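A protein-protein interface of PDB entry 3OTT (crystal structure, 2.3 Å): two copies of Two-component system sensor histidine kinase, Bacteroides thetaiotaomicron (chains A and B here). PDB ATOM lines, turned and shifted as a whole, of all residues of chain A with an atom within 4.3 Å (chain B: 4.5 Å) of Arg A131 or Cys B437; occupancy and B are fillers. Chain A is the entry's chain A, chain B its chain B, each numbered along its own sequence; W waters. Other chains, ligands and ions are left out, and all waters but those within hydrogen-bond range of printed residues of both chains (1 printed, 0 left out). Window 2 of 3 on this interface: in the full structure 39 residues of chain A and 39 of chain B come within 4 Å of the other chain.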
ATOM      1  N   PRO A  97     -35.992  20.455  15.210  1.00  0.00           N
ATOM      2  CA  PRO A  97     -34.757  20.822  15.910  1.00  0.00           C
ATOM      3  C   PRO A  97     -35.071  21.110  17.395  1.00  0.00           C
ATOM      4  O   PRO A  97     -36.234  21.396  17.720  1.00  0.00           O
ATOM      5  CB  PRO A  97     -34.282  22.091  15.171  1.00  0.00           C
ATOM      6  CG  PRO A  97     -35.351  22.465  14.159  1.00  0.00           C
ATOM      7  CD  PRO A  97     -36.539  21.561  14.404  1.00  0.00           C
ATOM      8  N   THR A  99     -34.601  23.613  19.225  1.00  0.00           N
ATOM      9  CA  THR A  99     -35.046  24.990  19.446  1.00  0.00           C
ATOM     10  C   THR A  99     -36.419  25.127  20.126  1.00  0.00           C
ATOM     11  O   THR A  99     -37.361  24.389  19.813  1.00  0.00           O
ATOM     12  CB  THR A  99     -35.086  25.774  18.139  1.00  0.00           C
ATOM     13  OG1 THR A  99     -33.928  25.448  17.358  1.00  0.00           O
ATOM     14  CG2 THR A  99     -35.110  27.266  18.440  1.00  0.00           C
ATOM     15  N   TYR A 126     -33.974  33.895  13.582  1.00  0.00           N
ATOM     16  CA  TYR A 126     -33.527  32.558  13.865  1.00  0.00           C
ATOM     17  C   TYR A 126     -32.384  32.331  12.902  1.00  0.00           C
ATOM     18  O   TYR A 126     -32.610  32.141  11.683  1.00  0.00           O
ATOM     19  CB  TYR A 126     -34.639  31.549  13.529  1.00  0.00           C
ATOM     20  CG  TYR A 126     -34.268  30.108  13.873  1.00  0.00           C
ATOM     21  CD1 TYR A 126     -33.914  29.760  15.176  1.00  0.00           C
ATOM     22  CD2 TYR A 126     -34.270  29.117  12.910  1.00  0.00           C
ATOM     23  CE1 TYR A 126     -33.578  28.448  15.498  1.00  0.00           C
ATOM     24  CE2 TYR A 126     -33.896  27.811  13.211  1.00  0.00           C
ATOM     25  CZ  TYR A 126     -33.574  27.477  14.509  1.00  0.00           C
ATOM     26  OH  TYR A 126     -33.249  26.175  14.870  1.00  0.00           O
ATOM     27  N   GLN A 127     -31.163  32.323  13.437  1.00  0.00           N
ATOM     28  CA  GLN A 127     -29.983  32.024  12.643  1.00  0.00           C
ATOM     29  C   GLN A 127     -29.905  30.503  12.416  1.00  0.00           C
ATOM     30  O   GLN A 127     -29.841  29.733  13.350  1.00  0.00           O
ATOM     31  CB  GLN A 127     -28.744  32.560  13.378  1.00  0.00           C
ATOM     32  CG  GLN A 127     -27.647  33.159  12.456  1.00  0.00           C
ATOM     33  CD  GLN A 127     -26.957  32.067  11.596  1.00  0.00           C
ATOM     34  OE1 GLN A 127     -26.766  30.943  12.033  1.00  0.00           O
ATOM     35  NE2 GLN A 127     -26.590  32.416  10.398  1.00  0.00           N
ATOM     36  N   LEU A 128     -29.911  30.086  11.170  1.00  0.00           N
ATOM     37  CA  LEU A 128     -30.089  28.687  10.818  1.00  0.00           C
ATOM     38  C   LEU A 128     -28.923  27.763  11.130  1.00  0.00           C
ATOM     39  O   LEU A 128     -29.178  26.557  11.325  1.00  0.00           O
ATOM     40  CB  LEU A 128     -30.534  28.510   9.365  1.00  0.00           C
ATOM     41  CG  LEU A 128     -31.972  29.089   9.072  1.00  0.00           C
ATOM     42  CD1 LEU A 128     -32.189  29.419   7.590  1.00  0.00           C
ATOM     43  CD2 LEU A 128     -33.093  28.241   9.573  1.00  0.00           C
ATOM     44  N   GLN A 129     -27.677  28.285  11.123  1.00  0.00           N
ATOM     45  CA  GLN A 129     -26.495  27.467  11.439  1.00  0.00           C
ATOM     46  C   GLN A 129     -26.302  27.294  12.946  1.00  0.00           C
ATOM     47  O   GLN A 129     -26.039  26.214  13.398  1.00  0.00           O
ATOM     48  CB  GLN A 129     -25.221  28.080  10.807  1.00  0.00           C
ATOM     49  CG  GLN A 129     -23.977  27.189  10.798  1.00  0.00           C
ATOM     50  CD  GLN A 129     -24.051  26.079   9.756  1.00  0.00           C
ATOM     51  OE1 GLN A 129     -25.089  25.884   9.105  1.00  0.00           O
ATOM     52  NE2 GLN A 129     -22.956  25.359   9.572  1.00  0.00           N
ATOM     53  N   SER A 130     -26.430  28.357  13.718  1.00  0.00           N
ATOM     54  CA  SER A 130     -26.089  28.312  15.126  1.00  0.00           C
ATOM     55  C   SER A 130     -27.333  28.073  15.946  1.00  0.00           C
ATOM     56  O   SER A 130     -27.233  27.828  17.134  1.00  0.00           O
ATOM     57  CB  SER A 130     -25.505  29.647  15.582  1.00  0.00           C
ATOM     58  OG  SER A 130     -26.531  30.628  15.479  1.00  0.00           O
ATOM     59  N   ARG A 131     -28.497  28.172  15.311  1.00  0.00           N
ATOM     60  CA  ARG A 131     -29.810  28.130  16.020  1.00  0.00           C
ATOM     61  C   ARG A 131     -30.050  29.305  16.997  1.00  0.00           C
ATOM     62  O   ARG A 131     -30.796  29.197  17.932  1.00  0.00           O
ATOM     63  CB  ARG A 131     -29.965  26.801  16.763  1.00  0.00           C
ATOM     64  CG  ARG A 131     -30.102  25.566  15.857  1.00  0.00           C
ATOM     65  CD  ARG A 131     -29.896  24.293  16.761  1.00  0.00           C
ATOM     66  NE  ARG A 131     -30.531  23.096  16.211  1.00  0.00           N
ATOM     67  CZ  ARG A 131     -29.921  21.914  16.037  1.00  0.00           C
ATOM     68  NH1 ARG A 131     -28.640  21.758  16.374  1.00  0.00           N
ATOM     69  NH2 ARG A 131     -30.596  20.864  15.543  1.00  0.00           N
ATOM     70  N   LYS A 132     -29.392  30.423  16.784  1.00  0.00           N
ATOM     71  CA  LYS A 132     -29.502  31.550  17.687  1.00  0.00           C
ATOM     72  C   LYS A 132     -30.825  32.255  17.485  1.00  0.00           C
ATOM     73  O   LYS A 132     -31.047  32.799  16.434  1.00  0.00           O
ATOM     74  CB  LYS A 132     -28.326  32.499  17.425  1.00  0.00           C
ATOM     75  CG  LYS A 132     -28.350  33.834  18.164  1.00  0.00           C
ATOM     76  CD  LYS A 132     -27.992  33.593  19.614  1.00  0.00           C
ATOM     77  CE  LYS A 132     -28.082  34.873  20.452  1.00  0.00           C
ATOM     78  NZ  LYS A 132     -27.919  34.421  21.872  1.00  0.00           N
ATOM     79  N   LEU A 133     -31.661  32.302  18.519  1.00  0.00           N
ATOM     80  CA  LEU A 133     -33.008  32.973  18.473  1.00  0.00           C
ATOM     81  C   LEU A 133     -32.913  34.334  19.178  1.00  0.00           C
ATOM     82  O   LEU A 133     -32.542  34.399  20.357  1.00  0.00           O
ATOM     83  CB  LEU A 133     -34.088  32.083  19.127  1.00  0.00           C
ATOM     84  CG  LEU A 133     -35.583  32.465  18.947  1.00  0.00           C
ATOM     85  CD1 LEU A 133     -36.130  32.195  17.537  1.00  0.00           C
ATOM     86  CD2 LEU A 133     -36.488  31.768  19.961  1.00  0.00           C
ATOM     87  N   TRP B 420     -26.854  14.272  12.046  1.00  0.00           N
ATOM     88  CA  TRP B 420     -26.422  15.640  12.270  1.00  0.00           C
ATOM     89  C   TRP B 420     -24.996  15.700  12.797  1.00  0.00           C
ATOM     90  O   TRP B 420     -24.790  15.721  13.984  1.00  0.00           O
ATOM     91  CB  TRP B 420     -27.398  16.349  13.234  1.00  0.00           C
ATOM     92  CG  TRP B 420     -28.816  16.455  12.675  1.00  0.00           C
ATOM     93  CD1 TRP B 420     -29.212  16.253  11.361  1.00  0.00           C
ATOM     94  CD2 TRP B 420     -30.003  16.809  13.401  1.00  0.00           C
ATOM     95  NE1 TRP B 420     -30.557  16.476  11.246  1.00  0.00           N
ATOM     96  CE2 TRP B 420     -31.070  16.829  12.470  1.00  0.00           C
ATOM     97  CE3 TRP B 420     -30.265  17.143  14.746  1.00  0.00           C
ATOM     98  CZ2 TRP B 420     -32.400  17.144  12.844  1.00  0.00           C
ATOM     99  CZ3 TRP B 420     -31.591  17.468  15.124  1.00  0.00           C
ATOM    100  CH2 TRP B 420     -32.642  17.461  14.165  1.00  0.00           C
ATOM    101  N   TYR B 422     -21.300  17.543  13.332  1.00  0.00           N
ATOM    102  CA  TYR B 422     -20.777  18.913  13.504  1.00  0.00           C
ATOM    103  C   TYR B 422     -19.293  19.001  13.316  1.00  0.00           C
ATOM    104  O   TYR B 422     -18.840  20.065  12.915  1.00  0.00           O
ATOM    105  CB  TYR B 422     -21.110  19.551  14.895  1.00  0.00           C
ATOM    106  CG  TYR B 422     -22.530  20.092  14.902  1.00  0.00           C
ATOM    107  CD1 TYR B 422     -23.618  19.234  14.667  1.00  0.00           C
ATOM    108  CD2 TYR B 422     -22.786  21.467  15.061  1.00  0.00           C
ATOM    109  CE1 TYR B 422     -24.949  19.721  14.624  1.00  0.00           C
ATOM    110  CE2 TYR B 422     -24.133  21.962  15.014  1.00  0.00           C
ATOM    111  CZ  TYR B 422     -25.186  21.078  14.799  1.00  0.00           C
ATOM    112  OH  TYR B 422     -26.483  21.528  14.762  1.00  0.00           O
ATOM    113  N   THR B 436     -21.609  14.909  17.118  1.00  0.00           N
ATOM    114  CA  THR B 436     -22.958  14.995  16.622  1.00  0.00           C
ATOM    115  C   THR B 436     -23.870  15.963  17.469  1.00  0.00           C
ATOM    116  O   THR B 436     -23.581  16.285  18.605  1.00  0.00           O
ATOM    117  CB  THR B 436     -23.472  13.543  16.683  1.00  0.00           C
ATOM    118  OG1 THR B 436     -22.863  12.808  15.597  1.00  0.00           O
ATOM    119  CG2 THR B 436     -24.875  13.458  16.513  1.00  0.00           C
ATOM    120  N   CYS B 437     -24.997  16.383  16.913  1.00  0.00           N
ATOM    121  CA  CYS B 437     -26.074  16.893  17.718  1.00  0.00           C
ATOM    122  C   CYS B 437     -26.963  15.663  18.016  1.00  0.00           C
ATOM    123  O   CYS B 437     -27.235  14.846  17.111  1.00  0.00           O
ATOM    124  CB  CYS B 437     -26.840  17.969  16.926  1.00  0.00           C
ATOM    125  SG  CYS B 437     -28.427  18.553  17.632  1.00  0.00           S
ATOM    126  N   LEU B 438     -27.348  15.473  19.265  1.00  0.00           N
ATOM    127  CA  LEU B 438     -28.261  14.373  19.677  1.00  0.00           C
ATOM    128  C   LEU B 438     -27.656  12.976  19.856  1.00  0.00           C
ATOM    129  O   LEU B 438     -28.189  12.183  20.631  1.00  0.00           O
ATOM    130  CB  LEU B 438     -29.521  14.243  18.799  1.00  0.00           C
ATOM    131  CG  LEU B 438     -30.643  15.299  18.828  1.00  0.00           C
ATOM    132  CD1 LEU B 438     -31.678  14.823  17.757  1.00  0.00           C
ATOM    133  CD2 LEU B 438     -31.323  15.452  20.187  1.00  0.00           C
ATOM    134  N   GLY B 439     -26.547  12.665  19.182  1.00  0.00           N
ATOM    135  CA  GLY B 439     -25.933  11.353  19.389  1.00  0.00           C
ATOM    136  C   GLY B 439     -24.608  11.348  20.135  1.00  0.00           C
ATOM    137  O   GLY B 439     -23.883  10.364  20.121  1.00  0.00           O
ATOM    138  N   MET B 472     -25.531  15.995  25.057  1.00  0.00           N
ATOM    139  CA  MET B 472     -25.589  15.197  23.831  1.00  0.00           C
ATOM    140  C   MET B 472     -25.369  16.037  22.564  1.00  0.00           C
ATOM    141  O   MET B 472     -25.152  15.460  21.470  1.00  0.00           O
ATOM    142  CB  MET B 472     -26.890  14.401  23.739  1.00  0.00           C
ATOM    143  CG  MET B 472     -26.977  13.238  24.757  1.00  0.00           C
ATOM    144  SD  MET B 472     -25.643  12.002  24.535  1.00  0.00           S
ATOM    145  CE  MET B 472     -26.161  11.106  23.107  1.00  0.00           C
ATOM    146  N   PHE B 473     -25.405  17.369  22.733  1.00  0.00           N
ATOM    147  CA  PHE B 473     -25.136  18.333  21.657  1.00  0.00           C
ATOM    148  C   PHE B 473     -23.711  18.836  21.689  1.00  0.00           C
ATOM    149  O   PHE B 473     -23.324  19.737  22.481  1.00  0.00           O
ATOM    150  CB  PHE B 473     -26.110  19.508  21.667  1.00  0.00           C
ATOM    151  CG  PHE B 473     -27.424  19.157  22.280  1.00  0.00           C
ATOM    152  CD1 PHE B 473     -28.524  18.829  21.467  1.00  0.00           C
ATOM    153  CD2 PHE B 473     -27.552  19.074  23.678  1.00  0.00           C
ATOM    154  CE1 PHE B 473     -29.748  18.463  22.027  1.00  0.00           C
ATOM    155  CE2 PHE B 473     -28.760  18.704  24.262  1.00  0.00           C
ATOM    156  CZ  PHE B 473     -29.874  18.406  23.430  1.00  0.00           C
ATOM    157  N   TYR B 490     -22.904  22.444  23.258  1.00  0.00           N
ATOM    158  CA  TYR B 490     -23.778  23.587  22.982  1.00  0.00           C
ATOM    159  C   TYR B 490     -24.401  24.063  24.313  1.00  0.00           C
ATOM    160  O   TYR B 490     -24.929  23.249  25.107  1.00  0.00           O
ATOM    161  CB  TYR B 490     -24.839  23.179  21.952  1.00  0.00           C
ATOM    162  CG  TYR B 490     -25.923  24.224  21.662  1.00  0.00           C
ATOM    163  CD1 TYR B 490     -25.649  25.355  20.860  1.00  0.00           C
ATOM    164  CD2 TYR B 490     -27.239  24.089  22.185  1.00  0.00           C
ATOM    165  CE1 TYR B 490     -26.634  26.324  20.578  1.00  0.00           C
ATOM    166  CE2 TYR B 490     -28.253  25.073  21.907  1.00  0.00           C
ATOM    167  CZ  TYR B 490     -27.931  26.174  21.085  1.00  0.00           C
ATOM    168  OH  TYR B 490     -28.887  27.146  20.797  1.00  0.00           O
HETATM  169  O   HOH W   1     -26.660  24.139  15.357  1.00  0.00           O
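No position is printed for both chains.
The guanidinium group (NH1) of Arg A131 sits at hydrogen-bond distance from the side-chain sulfur (SG) of Cys B437, 3.4 Å away. NH1 of Arg A131 is in hydrogen-bond range of OH of Tyr B422 (2.7 Å).
Among the printed residues, merely in contact across the chains: Arg A131 with Trp B420 and Ser A130 with Tyr B490.
Water W1 lies within hydrogen-bond range of the side-chain hydroxyl of Tyr B422, the backbone carbonyl oxygen of Gln A129 and the guanidinium group of Arg A131.
Printed residues of chain B within 4 Å of Arg A131: Trp B420, Tyr B422 and Cys B437. Printed residues of chain A within 4 Å of Tyr B422: Arg A131. Printed residues of chain A within 4 Å of Trp B420: Arg A131. Of the printed residues of chain B, Ser A130 touches Tyr B490. Gln A127 touches none of the printed residues of chain B. Pro A97 touches none of the printed residues of chain B. The nearest printed residue of chain B that does not touch Arg A131 is Tyr B490 (4.01 Å).
N of Lys A132 lies within hydrogen-bond range of OG of Ser A130. The side-chain amide oxygen (OE1) of Gln A127 is in hydrogen-bond range of the backbone NH (N) of Ser A130, at 3.1 Å. The backbone carbonyl oxygen (O) of Phe B473 is in hydrogen-bond range of the backbone NH (N) of Tyr B490, 2.8 Å away. The backbone carbonyl oxygen (O) of Trp B420 sits at hydrogen-bond distance from the backbone NH (N) of Cys B437 (3.0 Å).
Hydrophobic or aromatic side chains of chain B within 4 Å of the printed part of chain A: Trp B420, Tyr B422 and Tyr B490. Along chain B the printed residues that touch a printed residue of chain A span positions 420 to 490. Among the printed residues, 4 pairs touch across the chains.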
